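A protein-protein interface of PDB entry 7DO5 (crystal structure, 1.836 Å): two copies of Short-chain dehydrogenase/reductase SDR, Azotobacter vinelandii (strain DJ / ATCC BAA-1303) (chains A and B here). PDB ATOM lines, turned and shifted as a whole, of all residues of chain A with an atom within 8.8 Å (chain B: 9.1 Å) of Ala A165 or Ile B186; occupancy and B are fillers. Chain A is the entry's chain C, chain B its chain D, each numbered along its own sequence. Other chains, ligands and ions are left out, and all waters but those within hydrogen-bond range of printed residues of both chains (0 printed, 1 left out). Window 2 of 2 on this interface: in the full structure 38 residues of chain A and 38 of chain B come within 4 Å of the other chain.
CD1 of Phe A113 touches OH of Tyr B133, at 3.3 Å.
Phe A113 touches Cys B184 (CE2 to SG, 3.8 Å).
OH of Tyr B133 touches CG of Met A116 (3.4 Å).
Gln B182 touches Val A162.
Gly A163 touches Ile B186 (C to CD1, 3.3 Å).
CB of Ala A165 touches CG2 of Ile B186, 3.7 Å away.
Gln A167 touches Ser B183 (O to OG, 3.98 Å).
Thr A168 touches Leu B180 (O to CD1, 3.7 Å).
Ser B183 touches Thr A168 (CB to CG2, 3.8 Å).
His A169 touches Tyr B133 (N to OH, 3.9 Å).
N of Gly A164 lies within hydrogen-bond range of OG of Ser B183, at 2.9 Å.
OG1 of Thr A171 sits at hydrogen-bond distance from OG of Ser B179.
The side-chain hydroxyl (OG1) of Thr A171 lies within hydrogen-bond range of the side-chain hydroxyl (OG) of Ser B183, at 2.8 Å.
OG1 of Thr A168 lies within hydrogen-bond range of OH of Tyr B133, 2.7 Å away.
Printed residues of chain B within 4 Å of Phe A113: Tyr B133 and Cys B184.
Of the printed residues of chain B, Met A116 touches Tyr B133.
Of chain B, only Ser B183 and Ile B186 come within 4 Å of Gly A163.
Of chain B, only Ser B183 (2.9 Å) and Ile B186 (3.5 Å) come within 4 Å of Gly A164.
Of chain B, only Ile B186 and Ala B187 come within 4 Å of Ala A165.
Ile B186 touches just these residues of chain A: Gly A163 (3.3 Å), Gly A164 (3.5 Å) and Ala A165 (3.7 Å).
Printed residues of chain A within 4 Å of Ala B187: Ala A165.
Ala B254 touches none of the printed residues of chain A.
The nearest residue of chain B that does not touch Ala A165 is Ser B183 (4.1 Å).
The nearest residue of chain A that does not touch Ile B186 is Val A162 (5.6 Å).
The backbone carbonyl oxygen (O) of Leu B180 sits close to the side-chain sulfur (SG) of Cys B184, 3.3 Å away.
The backbone carbonyl oxygen (O) of Leu B188 is in hydrogen-bond range of the backbone NH (N) of Ile B193, at 3.4 Å.
No position is printed for both chains.
Of the 18 printed residues of chain A, 11 touch a printed residue of chain B.
Hydrophobic or aromatic side chains of chain A that line the printed part of chain B: Phe A113, Leu A114, Met A116 and Ala A165.
Of the 21 printed residues of chain B, 9 touch a printed residue of chain A.
Among the printed residues, 18 pairs touch across the chains.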
ATOM      1  N   PHE A 110      -0.912  -4.422 -24.539  1.00  0.00           N
ATOM      2  CA  PHE A 110      -2.345  -4.196 -24.380  1.00  0.00           C
ATOM      3  C   PHE A 110      -2.983  -5.317 -23.573  1.00  0.00           C
ATOM      4  O   PHE A 110      -2.687  -6.495 -23.782  1.00  0.00           O
ATOM      5  CB  PHE A 110      -3.016  -4.091 -25.754  1.00  0.00           C
ATOM      6  CG  PHE A 110      -2.586  -2.878 -26.544  1.00  0.00           C
ATOM      7  CD1 PHE A 110      -3.147  -1.634 -26.288  1.00  0.00           C
ATOM      8  CD2 PHE A 110      -1.621  -2.983 -27.537  1.00  0.00           C
ATOM      9  CE1 PHE A 110      -2.751  -0.517 -27.004  1.00  0.00           C
ATOM     10  CE2 PHE A 110      -1.222  -1.864 -28.257  1.00  0.00           C
ATOM     11  CZ  PHE A 110      -1.786  -0.630 -27.986  1.00  0.00           C
ATOM     12  N   HIS A 111      -3.858  -4.941 -22.640  1.00  0.00           N
ATOM     13  CA  HIS A 111      -4.473  -5.916 -21.745  1.00  0.00           C
ATOM     14  C   HIS A 111      -5.645  -5.256 -21.037  1.00  0.00           C
ATOM     15  O   HIS A 111      -5.551  -4.090 -20.642  1.00  0.00           O
ATOM     16  CB  HIS A 111      -3.462  -6.437 -20.712  1.00  0.00           C
ATOM     17  CG  HIS A 111      -3.842  -7.743 -20.082  1.00  0.00           C
ATOM     18  ND1 HIS A 111      -4.865  -7.862 -19.165  1.00  0.00           N
ATOM     19  CD2 HIS A 111      -3.342  -8.991 -20.248  1.00  0.00           C
ATOM     20  CE1 HIS A 111      -4.978  -9.123 -18.789  1.00  0.00           C
ATOM     21  NE2 HIS A 111      -4.062  -9.829 -19.426  1.00  0.00           N
ATOM     22  N   SER A 112      -6.730  -6.006 -20.858  1.00  0.00           N
ATOM     23  CA  SER A 112      -7.886  -5.463 -20.153  1.00  0.00           C
ATOM     24  C   SER A 112      -7.562  -5.220 -18.675  1.00  0.00           C
ATOM     25  O   SER A 112      -6.623  -5.792 -18.109  1.00  0.00           O
ATOM     26  CB  SER A 112      -9.094  -6.389 -20.300  1.00  0.00           C
ATOM     27  OG  SER A 112      -8.721  -7.756 -20.235  1.00  0.00           O
ATOM     28  N   PHE A 113      -8.365  -4.346 -18.053  1.00  0.00           N
ATOM     29  CA  PHE A 113      -8.063  -3.852 -16.713  1.00  0.00           C
ATOM     30  C   PHE A 113      -8.434  -4.860 -15.629  1.00  0.00           C
ATOM     31  O   PHE A 113      -7.637  -5.123 -14.721  1.00  0.00           O
ATOM     32  CB  PHE A 113      -8.797  -2.525 -16.468  1.00  0.00           C
ATOM     33  CG  PHE A 113      -8.713  -2.035 -15.046  1.00  0.00           C
ATOM     34  CD1 PHE A 113      -7.482  -1.848 -14.433  1.00  0.00           C
ATOM     35  CD2 PHE A 113      -9.865  -1.754 -14.325  1.00  0.00           C
ATOM     36  CE1 PHE A 113      -7.407  -1.385 -13.125  1.00  0.00           C
ATOM     37  CE2 PHE A 113      -9.798  -1.290 -13.024  1.00  0.00           C
ATOM     38  CZ  PHE A 113      -8.578  -1.113 -12.420  1.00  0.00           C
ATOM     39  N   LEU A 114      -9.646  -5.422 -15.692  1.00  0.00           N
ATOM     40  CA  LEU A 114     -10.151  -6.158 -14.533  1.00  0.00           C
ATOM     41  C   LEU A 114      -9.366  -7.435 -14.271  1.00  0.00           C
ATOM     42  O   LEU A 114      -9.327  -7.899 -13.126  1.00  0.00           O
ATOM     43  CB  LEU A 114     -11.638  -6.463 -14.705  1.00  0.00           C
ATOM     44  CG  LEU A 114     -12.517  -5.215 -14.538  1.00  0.00           C
ATOM     45  CD1 LEU A 114     -13.963  -5.521 -14.855  1.00  0.00           C
ATOM     46  CD2 LEU A 114     -12.376  -4.606 -13.135  1.00  0.00           C
ATOM     47  N   ASP A 115      -8.717  -8.001 -15.290  1.00  0.00           N
ATOM     48  CA  ASP A 115      -7.883  -9.187 -15.114  1.00  0.00           C
ATOM     49  C   ASP A 115      -6.394  -8.902 -15.321  1.00  0.00           C
ATOM     50  O   ASP A 115      -5.627  -9.828 -15.600  1.00  0.00           O
ATOM     51  CB  ASP A 115      -8.334 -10.294 -16.063  1.00  0.00           C
ATOM     52  CG  ASP A 115      -8.205  -9.893 -17.506  1.00  0.00           C
ATOM     53  OD1 ASP A 115      -8.102  -8.675 -17.783  1.00  0.00           O
ATOM     54  OD2 ASP A 115      -8.212 -10.794 -18.367  1.00  0.00           O
ATOM     55  N   MET A 116      -5.975  -7.643 -15.194  1.00  0.00           N
ATOM     56  CA  MET A 116      -4.569  -7.289 -15.336  1.00  0.00           C
ATOM     57  C   MET A 116      -3.715  -8.024 -14.313  1.00  0.00           C
ATOM     58  O   MET A 116      -3.911  -7.834 -13.103  1.00  0.00           O
ATOM     59  CB  MET A 116      -4.355  -5.784 -15.164  1.00  0.00           C
ATOM     60  CG  MET A 116      -2.870  -5.403 -15.176  1.00  0.00           C
ATOM     61  SD  MET A 116      -2.187  -5.416 -16.861  1.00  0.00           S
ATOM     62  CE  MET A 116      -3.304  -4.298 -17.700  1.00  0.00           C
ATOM     63  N   SER A 159      -1.439   9.459 -25.348  1.00  0.00           N
ATOM     64  CA  SER A 159      -2.094   8.785 -24.232  1.00  0.00           C
ATOM     65  C   SER A 159      -1.728   9.372 -22.882  1.00  0.00           C
ATOM     66  O   SER A 159      -2.265   8.909 -21.865  1.00  0.00           O
ATOM     67  CB  SER A 159      -1.748   7.287 -24.228  1.00  0.00           C
ATOM     68  OG  SER A 159      -2.274   6.654 -25.383  1.00  0.00           O
ATOM     69  N   VAL A 162      -5.229  11.447 -22.458  1.00  0.00           N
ATOM     70  CA  VAL A 162      -6.521  10.804 -22.621  1.00  0.00           C
ATOM     71  C   VAL A 162      -6.376   9.360 -22.161  1.00  0.00           C
ATOM     72  O   VAL A 162      -5.294   8.922 -21.765  1.00  0.00           O
ATOM     73  CB  VAL A 162      -7.028  10.858 -24.079  1.00  0.00           C
ATOM     74  CG1 VAL A 162      -7.337  12.304 -24.505  1.00  0.00           C
ATOM     75  CG2 VAL A 162      -5.996  10.229 -25.013  1.00  0.00           C
ATOM     76  N   GLY A 163      -7.482   8.614 -22.216  1.00  0.00           N
ATOM     77  CA  GLY A 163      -7.511   7.260 -21.715  1.00  0.00           C
ATOM     78  C   GLY A 163      -7.432   6.216 -22.814  1.00  0.00           C
ATOM     79  O   GLY A 163      -7.507   6.516 -24.002  1.00  0.00           O
ATOM     80  N   GLY A 164      -7.311   4.962 -22.374  1.00  0.00           N
ATOM     81  CA  GLY A 164      -7.436   3.796 -23.237  1.00  0.00           C
ATOM     82  C   GLY A 164      -7.833   2.584 -22.406  1.00  0.00           C
ATOM     83  O   GLY A 164      -7.158   2.269 -21.422  1.00  0.00           O
ATOM     84  N   ALA A 165      -8.935   1.925 -22.769  1.00  0.00           N
ATOM     85  CA  ALA A 165      -9.471   0.827 -21.960  1.00  0.00           C
ATOM     86  C   ALA A 165      -8.479  -0.322 -21.801  1.00  0.00           C
ATOM     87  O   ALA A 165      -8.462  -0.990 -20.755  1.00  0.00           O
ATOM     88  CB  ALA A 165     -10.767   0.300 -22.582  1.00  0.00           C
ATOM     89  N   MET A 166      -7.667  -0.582 -22.826  1.00  0.00           N
ATOM     90  CA  MET A 166      -6.679  -1.650 -22.798  1.00  0.00           C
ATOM     91  C   MET A 166      -5.308  -1.139 -22.400  1.00  0.00           C
ATOM     92  O   MET A 166      -4.313  -1.843 -22.598  1.00  0.00           O
ATOM     93  CB  MET A 166      -6.602  -2.343 -24.163  1.00  0.00           C
ATOM     94  CG  MET A 166      -7.936  -2.913 -24.617  1.00  0.00           C
ATOM     95  SD  MET A 166      -8.367  -4.334 -23.629  1.00  0.00           S
ATOM     96  CE  MET A 166      -7.210  -5.516 -24.305  1.00  0.00           C
ATOM     97  N   GLN A 167      -5.239   0.073 -21.841  1.00  0.00           N
ATOM     98  CA  GLN A 167      -3.984   0.720 -21.481  1.00  0.00           C
ATOM     99  C   GLN A 167      -4.059   1.328 -20.088  1.00  0.00           C
ATOM    100  O   GLN A 167      -3.447   2.373 -19.833  1.00  0.00           O
ATOM    101  CB  GLN A 167      -3.610   1.806 -22.500  1.00  0.00           C
ATOM    102  CG  GLN A 167      -3.401   1.321 -23.919  1.00  0.00           C
ATOM    103  CD  GLN A 167      -3.382   2.466 -24.925  1.00  0.00           C
ATOM    104  OE1 GLN A 167      -4.405   3.093 -25.188  1.00  0.00           O
ATOM    105  NE2 GLN A 167      -2.212   2.748 -25.476  1.00  0.00           N
ATOM    106  N   THR A 168      -4.822   0.708 -19.175  1.00  0.00           N
ATOM    107  CA  THR A 168      -4.921   1.265 -17.827  1.00  0.00           C
ATOM    108  C   THR A 168      -3.577   1.251 -17.117  1.00  0.00           C
ATOM    109  O   THR A 168      -3.324   2.091 -16.254  1.00  0.00           O
ATOM    110  CB  THR A 168      -5.943   0.502 -16.983  1.00  0.00           C
ATOM    111  OG1 THR A 168      -5.649  -0.907 -17.021  1.00  0.00           O
ATOM    112  CG2 THR A 168      -7.364   0.784 -17.463  1.00  0.00           C
ATOM    113  N   HIS A 169      -2.725   0.293 -17.444  1.00  0.00           N
ATOM    114  CA  HIS A 169      -1.374   0.229 -16.905  1.00  0.00           C
ATOM    115  C   HIS A 169      -0.412   1.148 -17.638  1.00  0.00           C
ATOM    116  O   HIS A 169       0.657   1.461 -17.102  1.00  0.00           O
ATOM    117  CB  HIS A 169      -0.843  -1.208 -16.985  1.00  0.00           C
ATOM    118  CG  HIS A 169      -0.880  -1.792 -18.365  1.00  0.00           C
ATOM    119  ND1 HIS A 169      -1.922  -1.573 -19.242  1.00  0.00           N
ATOM    120  CD2 HIS A 169      -0.010  -2.602 -19.014  1.00  0.00           C
ATOM    121  CE1 HIS A 169      -1.696  -2.223 -20.371  1.00  0.00           C
ATOM    122  NE2 HIS A 169      -0.542  -2.860 -20.258  1.00  0.00           N
ATOM    123  N   TYR A 170      -0.759   1.572 -18.850  1.00  0.00           N
ATOM    124  CA  TYR A 170       0.156   2.283 -19.736  1.00  0.00           C
ATOM    125  C   TYR A 170      -0.011   3.796 -19.673  1.00  0.00           C
ATOM    126  O   TYR A 170       0.982   4.521 -19.513  1.00  0.00           O
ATOM    127  CB  TYR A 170      -0.062   1.799 -21.173  1.00  0.00           C
ATOM    128  CG  TYR A 170       0.714   2.543 -22.245  1.00  0.00           C
ATOM    129  CD1 TYR A 170       2.069   2.312 -22.436  1.00  0.00           C
ATOM    130  CD2 TYR A 170       0.074   3.448 -23.099  1.00  0.00           C
ATOM    131  CE1 TYR A 170       2.779   2.964 -23.426  1.00  0.00           C
ATOM    132  CE2 TYR A 170       0.779   4.103 -24.109  1.00  0.00           C
ATOM    133  CZ  TYR A 170       2.131   3.856 -24.258  1.00  0.00           C
ATOM    134  OH  TYR A 170       2.836   4.496 -25.252  1.00  0.00           O
ATOM    135  N   THR A 171      -1.240   4.297 -19.801  1.00  0.00           N
ATOM    136  CA  THR A 171      -1.409   5.751 -19.815  1.00  0.00           C
ATOM    137  C   THR A 171      -0.884   6.405 -18.542  1.00  0.00           C
ATOM    138  O   THR A 171      -0.316   7.500 -18.653  1.00  0.00           O
ATOM    139  CB  THR A 171      -2.873   6.161 -20.085  1.00  0.00           C
ATOM    140  OG1 THR A 171      -3.702   5.902 -18.943  1.00  0.00           O
ATOM    141  CG2 THR A 171      -3.450   5.421 -21.310  1.00  0.00           C
ATOM    142  N   TYR B 133      -3.761   1.323  -8.124  1.00  0.00           N
ATOM    143  CA  TYR B 133      -4.181   0.519  -9.271  1.00  0.00           C
ATOM    144  C   TYR B 133      -4.928  -0.738  -8.833  1.00  0.00           C
ATOM    145  O   TYR B 133      -6.021  -1.039  -9.328  1.00  0.00           O
ATOM    146  CB  TYR B 133      -2.962   0.142 -10.120  1.00  0.00           C
ATOM    147  CG  TYR B 133      -3.319  -0.507 -11.441  1.00  0.00           C
ATOM    148  CD1 TYR B 133      -3.574   0.266 -12.572  1.00  0.00           C
ATOM    149  CD2 TYR B 133      -3.409  -1.891 -11.552  1.00  0.00           C
ATOM    150  CE1 TYR B 133      -3.915  -0.315 -13.769  1.00  0.00           C
ATOM    151  CE2 TYR B 133      -3.752  -2.491 -12.754  1.00  0.00           C
ATOM    152  CZ  TYR B 133      -3.983  -1.694 -13.867  1.00  0.00           C
ATOM    153  OH  TYR B 133      -4.316  -2.284 -15.060  1.00  0.00           O
ATOM    154  N   SER B 179      -4.603   9.970 -14.850  1.00  0.00           N
ATOM    155  CA  SER B 179      -4.620   9.167 -16.068  1.00  0.00           C
ATOM    156  C   SER B 179      -5.318   7.827 -15.857  1.00  0.00           C
ATOM    157  O   SER B 179      -6.057   7.357 -16.734  1.00  0.00           O
ATOM    158  CB  SER B 179      -3.184   8.955 -16.554  1.00  0.00           C
ATOM    159  OG  SER B 179      -3.171   8.175 -17.733  1.00  0.00           O
ATOM    160  N   LEU B 180      -5.073   7.179 -14.713  1.00  0.00           N
ATOM    161  CA  LEU B 180      -5.769   5.932 -14.404  1.00  0.00           C
ATOM    162  C   LEU B 180      -7.281   6.120 -14.428  1.00  0.00           C
ATOM    163  O   LEU B 180      -8.002   5.297 -15.003  1.00  0.00           O
ATOM    164  CB  LEU B 180      -5.320   5.398 -13.039  1.00  0.00           C
ATOM    165  CG  LEU B 180      -5.951   4.082 -12.571  1.00  0.00           C
ATOM    166  CD1 LEU B 180      -5.652   2.963 -13.576  1.00  0.00           C
ATOM    167  CD2 LEU B 180      -5.440   3.706 -11.190  1.00  0.00           C
ATOM    168  N   MET B 181      -7.782   7.213 -13.836  1.00  0.00           N
ATOM    169  CA  MET B 181      -9.226   7.442 -13.848  1.00  0.00           C
ATOM    170  C   MET B 181      -9.739   7.653 -15.270  1.00  0.00           C
ATOM    171  O   MET B 181     -10.838   7.199 -15.615  1.00  0.00           O
ATOM    172  CB  MET B 181      -9.580   8.639 -12.954  1.00  0.00           C
ATOM    173  CG  MET B 181      -9.285   8.417 -11.464  1.00  0.00           C
ATOM    174  SD  MET B 181     -10.246   7.076 -10.698  1.00  0.00           S
ATOM    175  CE  MET B 181      -9.092   5.718 -10.848  1.00  0.00           C
ATOM    176  N   GLN B 182      -8.948   8.315 -16.121  1.00  0.00           N
ATOM    177  CA  GLN B 182      -9.376   8.499 -17.505  1.00  0.00           C
ATOM    178  C   GLN B 182      -9.497   7.161 -18.217  1.00  0.00           C
ATOM    179  O   GLN B 182     -10.475   6.914 -18.933  1.00  0.00           O
ATOM    180  CB  GLN B 182      -8.389   9.400 -18.251  1.00  0.00           C
ATOM    181  CG  GLN B 182      -8.235  10.820 -17.684  1.00  0.00           C
ATOM    182  CD  GLN B 182      -7.213  11.616 -18.480  1.00  0.00           C
ATOM    183  OE1 GLN B 182      -6.097  11.140 -18.725  1.00  0.00           O
ATOM    184  NE2 GLN B 182      -7.594  12.820 -18.904  1.00  0.00           N
ATOM    185  N   SER B 183      -8.513   6.278 -18.031  1.00  0.00           N
ATOM    186  CA  SER B 183      -8.559   5.000 -18.743  1.00  0.00           C
ATOM    187  C   SER B 183      -9.571   4.036 -18.129  1.00  0.00           C
ATOM    188  O   SER B 183     -10.265   3.316 -18.861  1.00  0.00           O
ATOM    189  CB  SER B 183      -7.161   4.387 -18.783  1.00  0.00           C
ATOM    190  OG  SER B 183      -6.336   5.111 -19.682  1.00  0.00           O
ATOM    191  N   CYS B 184      -9.668   3.997 -16.794  1.00  0.00           N
ATOM    192  CA  CYS B 184     -10.688   3.178 -16.142  1.00  0.00           C
ATOM    193  C   CYS B 184     -12.085   3.632 -16.511  1.00  0.00           C
ATOM    194  O   CYS B 184     -12.996   2.805 -16.596  1.00  0.00           O
ATOM    195  CB  CYS B 184     -10.531   3.206 -14.622  1.00  0.00           C
ATOM    196  SG  CYS B 184      -9.091   2.304 -14.057  1.00  0.00           S
ATOM    197  N   ALA B 185     -12.279   4.943 -16.703  1.00  0.00           N
ATOM    198  CA  ALA B 185     -13.578   5.463 -17.120  1.00  0.00           C
ATOM    199  C   ALA B 185     -14.045   4.799 -18.407  1.00  0.00           C
ATOM    200  O   ALA B 185     -15.238   4.529 -18.583  1.00  0.00           O
ATOM    201  CB  ALA B 185     -13.489   6.982 -17.304  1.00  0.00           C
ATOM    202  N   ILE B 186     -13.123   4.577 -19.338  1.00  0.00           N
ATOM    203  CA  ILE B 186     -13.470   3.899 -20.587  1.00  0.00           C
ATOM    204  C   ILE B 186     -13.738   2.418 -20.333  1.00  0.00           C
ATOM    205  O   ILE B 186     -14.722   1.843 -20.819  1.00  0.00           O
ATOM    206  CB  ILE B 186     -12.338   4.083 -21.614  1.00  0.00           C
ATOM    207  CG1 ILE B 186     -11.962   5.563 -21.739  1.00  0.00           C
ATOM    208  CG2 ILE B 186     -12.729   3.464 -22.967  1.00  0.00           C
ATOM    209  CD1 ILE B 186     -10.709   5.765 -22.563  1.00  0.00           C
ATOM    210  N   ALA B 187     -12.845   1.775 -19.592  1.00  0.00           N
ATOM    211  CA  ALA B 187     -12.941   0.335 -19.383  1.00  0.00           C
ATOM    212  C   ALA B 187     -14.180  -0.045 -18.578  1.00  0.00           C
ATOM    213  O   ALA B 187     -14.745  -1.127 -18.779  1.00  0.00           O
ATOM    214  CB  ALA B 187     -11.687  -0.163 -18.668  1.00  0.00           C
ATOM    215  N   LEU B 188     -14.623   0.820 -17.674  1.00  0.00           N
ATOM    216  CA  LEU B 188     -15.678   0.458 -16.740  1.00  0.00           C
ATOM    217  C   LEU B 188     -17.001   1.149 -17.026  1.00  0.00           C
ATOM    218  O   LEU B 188     -18.012   0.794 -16.397  1.00  0.00           O
ATOM    219  CB  LEU B 188     -15.241   0.768 -15.296  1.00  0.00           C
ATOM    220  CG  LEU B 188     -13.938   0.107 -14.830  1.00  0.00           C
ATOM    221  CD1 LEU B 188     -13.521   0.664 -13.481  1.00  0.00           C
ATOM    222  CD2 LEU B 188     -14.068  -1.430 -14.756  1.00  0.00           C
ATOM    223  N   GLY B 189     -17.017   2.127 -17.942  1.00  0.00           N
ATOM    224  CA  GLY B 189     -18.253   2.764 -18.345  1.00  0.00           C
ATOM    225  C   GLY B 189     -19.368   1.824 -18.745  1.00  0.00           C
ATOM    226  O   GLY B 189     -20.527   2.066 -18.384  1.00  0.00           O
ATOM    227  N   PRO B 190     -19.081   0.747 -19.491  1.00  0.00           N
ATOM    228  CA  PRO B 190     -20.154  -0.197 -19.850  1.00  0.00           C
ATOM    229  C   PRO B 190     -20.800  -0.880 -18.655  1.00  0.00           C
ATOM    230  O   PRO B 190     -21.877  -1.461 -18.807  1.00  0.00           O
ATOM    231  CB  PRO B 190     -19.435  -1.214 -20.747  1.00  0.00           C
ATOM    232  CG  PRO B 190     -18.285  -0.435 -21.331  1.00  0.00           C
ATOM    233  CD  PRO B 190     -17.832   0.440 -20.218  1.00  0.00           C
ATOM    234  N   TYR B 191     -20.183  -0.846 -17.478  1.00  0.00           N
ATOM    235  CA  TYR B 191     -20.768  -1.455 -16.291  1.00  0.00           C
ATOM    236  C   TYR B 191     -21.370  -0.425 -15.349  1.00  0.00           C
ATOM    237  O   TYR B 191     -21.666  -0.756 -14.201  1.00  0.00           O
ATOM    238  CB  TYR B 191     -19.725  -2.281 -15.553  1.00  0.00           C
ATOM    239  CG  TYR B 191     -18.932  -3.180 -16.466  1.00  0.00           C
ATOM    240  CD1 TYR B 191     -19.554  -4.212 -17.174  1.00  0.00           C
ATOM    241  CD2 TYR B 191     -17.565  -3.008 -16.623  1.00  0.00           C
ATOM    242  CE1 TYR B 191     -18.826  -5.043 -18.015  1.00  0.00           C
ATOM    243  CE2 TYR B 191     -16.828  -3.835 -17.455  1.00  0.00           C
ATOM    244  CZ  TYR B 191     -17.465  -4.850 -18.151  1.00  0.00           C
ATOM    245  OH  TYR B 191     -16.729  -5.671 -18.977  1.00  0.00           O
ATOM    246  N   GLY B 192     -21.558   0.807 -15.809  1.00  0.00           N
ATOM    247  CA  GLY B 192     -22.153   1.826 -14.974  1.00  0.00           C
ATOM    248  C   GLY B 192     -21.263   2.307 -13.857  1.00  0.00           C
ATOM    249  O   GLY B 192     -21.769   2.838 -12.866  1.00  0.00           O
ATOM    250  N   ILE B 193     -19.952   2.130 -13.977  1.00  0.00           N
ATOM    251  CA  ILE B 193     -18.998   2.584 -12.962  1.00  0.00           C
ATOM    252  C   ILE B 193     -18.346   3.873 -13.442  1.00  0.00           C
ATOM    253  O   ILE B 193     -17.661   3.878 -14.474  1.00  0.00           O
ATOM    254  CB  ILE B 193     -17.932   1.518 -12.678  1.00  0.00           C
ATOM    255  CG1 ILE B 193     -18.578   0.227 -12.154  1.00  0.00           C
ATOM    256  CG2 ILE B 193     -16.886   2.059 -11.686  1.00  0.00           C
ATOM    257  CD1 ILE B 193     -17.682  -1.013 -12.324  1.00  0.00           C
ATOM    258  N   ARG B 194     -18.519   4.956 -12.676  1.00  0.00           N
ATOM    259  CA  ARG B 194     -17.937   6.258 -12.991  1.00  0.00           C
ATOM    260  C   ARG B 194     -16.632   6.441 -12.215  1.00  0.00           C
ATOM    261  O   ARG B 194     -16.542   6.071 -11.036  1.00  0.00           O
ATOM    262  CB  ARG B 194     -18.918   7.391 -12.653  1.00  0.00           C
ATOM    263  CG  ARG B 194     -20.240   7.330 -13.434  1.00  0.00           C
ATOM    264  CD  ARG B 194     -21.194   8.477 -13.076  1.00  0.00           C
ATOM    265  NE  ARG B 194     -21.554   8.458 -11.664  1.00  0.00           N
ATOM    266  CZ  ARG B 194     -20.942   9.170 -10.718  1.00  0.00           C
ATOM    267  NH1 ARG B 194     -19.936   9.979 -11.031  1.00  0.00           N
ATOM    268  NH2 ARG B 194     -21.338   9.070  -9.460  1.00  0.00           N
ATOM    269  N   CYS B 195     -15.610   6.969 -12.896  1.00  0.00           N
ATOM    270  CA  CYS B 195     -14.260   7.131 -12.340  1.00  0.00           C
ATOM    271  C   CYS B 195     -13.814   8.574 -12.509  1.00  0.00           C
ATOM    272  O   CYS B 195     -13.751   9.067 -13.640  1.00  0.00           O
ATOM    273  CB  CYS B 195     -13.266   6.203 -13.030  1.00  0.00           C
ATOM    274  SG  CYS B 195     -13.787   4.486 -12.998  1.00  0.00           S
ATOM    275  N   THR B 252     -17.777  11.241 -15.714  1.00  0.00           N
ATOM    276  CA  THR B 252     -16.770  10.196 -15.589  1.00  0.00           C
ATOM    277  C   THR B 252     -15.602  10.568 -16.489  1.00  0.00           C
ATOM    278  O   THR B 252     -15.776  11.263 -17.494  1.00  0.00           O
ATOM    279  CB  THR B 252     -17.343   8.800 -15.929  1.00  0.00           C
ATOM    280  OG1 THR B 252     -16.360   7.785 -15.671  1.00  0.00           O
ATOM    281  CG2 THR B 252     -17.789   8.722 -17.399  1.00  0.00           C
ATOM    282  N   GLY B 253     -14.409  10.115 -16.110  1.00  0.00           N
ATOM    283  CA  GLY B 253     -13.202  10.559 -16.786  1.00  0.00           C
ATOM    284  C   GLY B 253     -12.870  12.029 -16.576  1.00  0.00           C
ATOM    285  O   GLY B 253     -12.153  12.612 -17.390  1.00  0.00           O
ATOM    286  N   ALA B 254     -13.378  12.645 -15.509  1.00  0.00           N
ATOM    287  CA  ALA B 254     -13.206  14.064 -15.261  1.00  0.00           C
ATOM    288  C   ALA B 254     -12.262  14.281 -14.088  1.00  0.00           C
ATOM    289  O   ALA B 254     -12.030  13.383 -13.275  1.00  0.00           O
ATOM    290  CB  ALA B 254     -14.547  14.747 -14.963  1.00  0.00           C
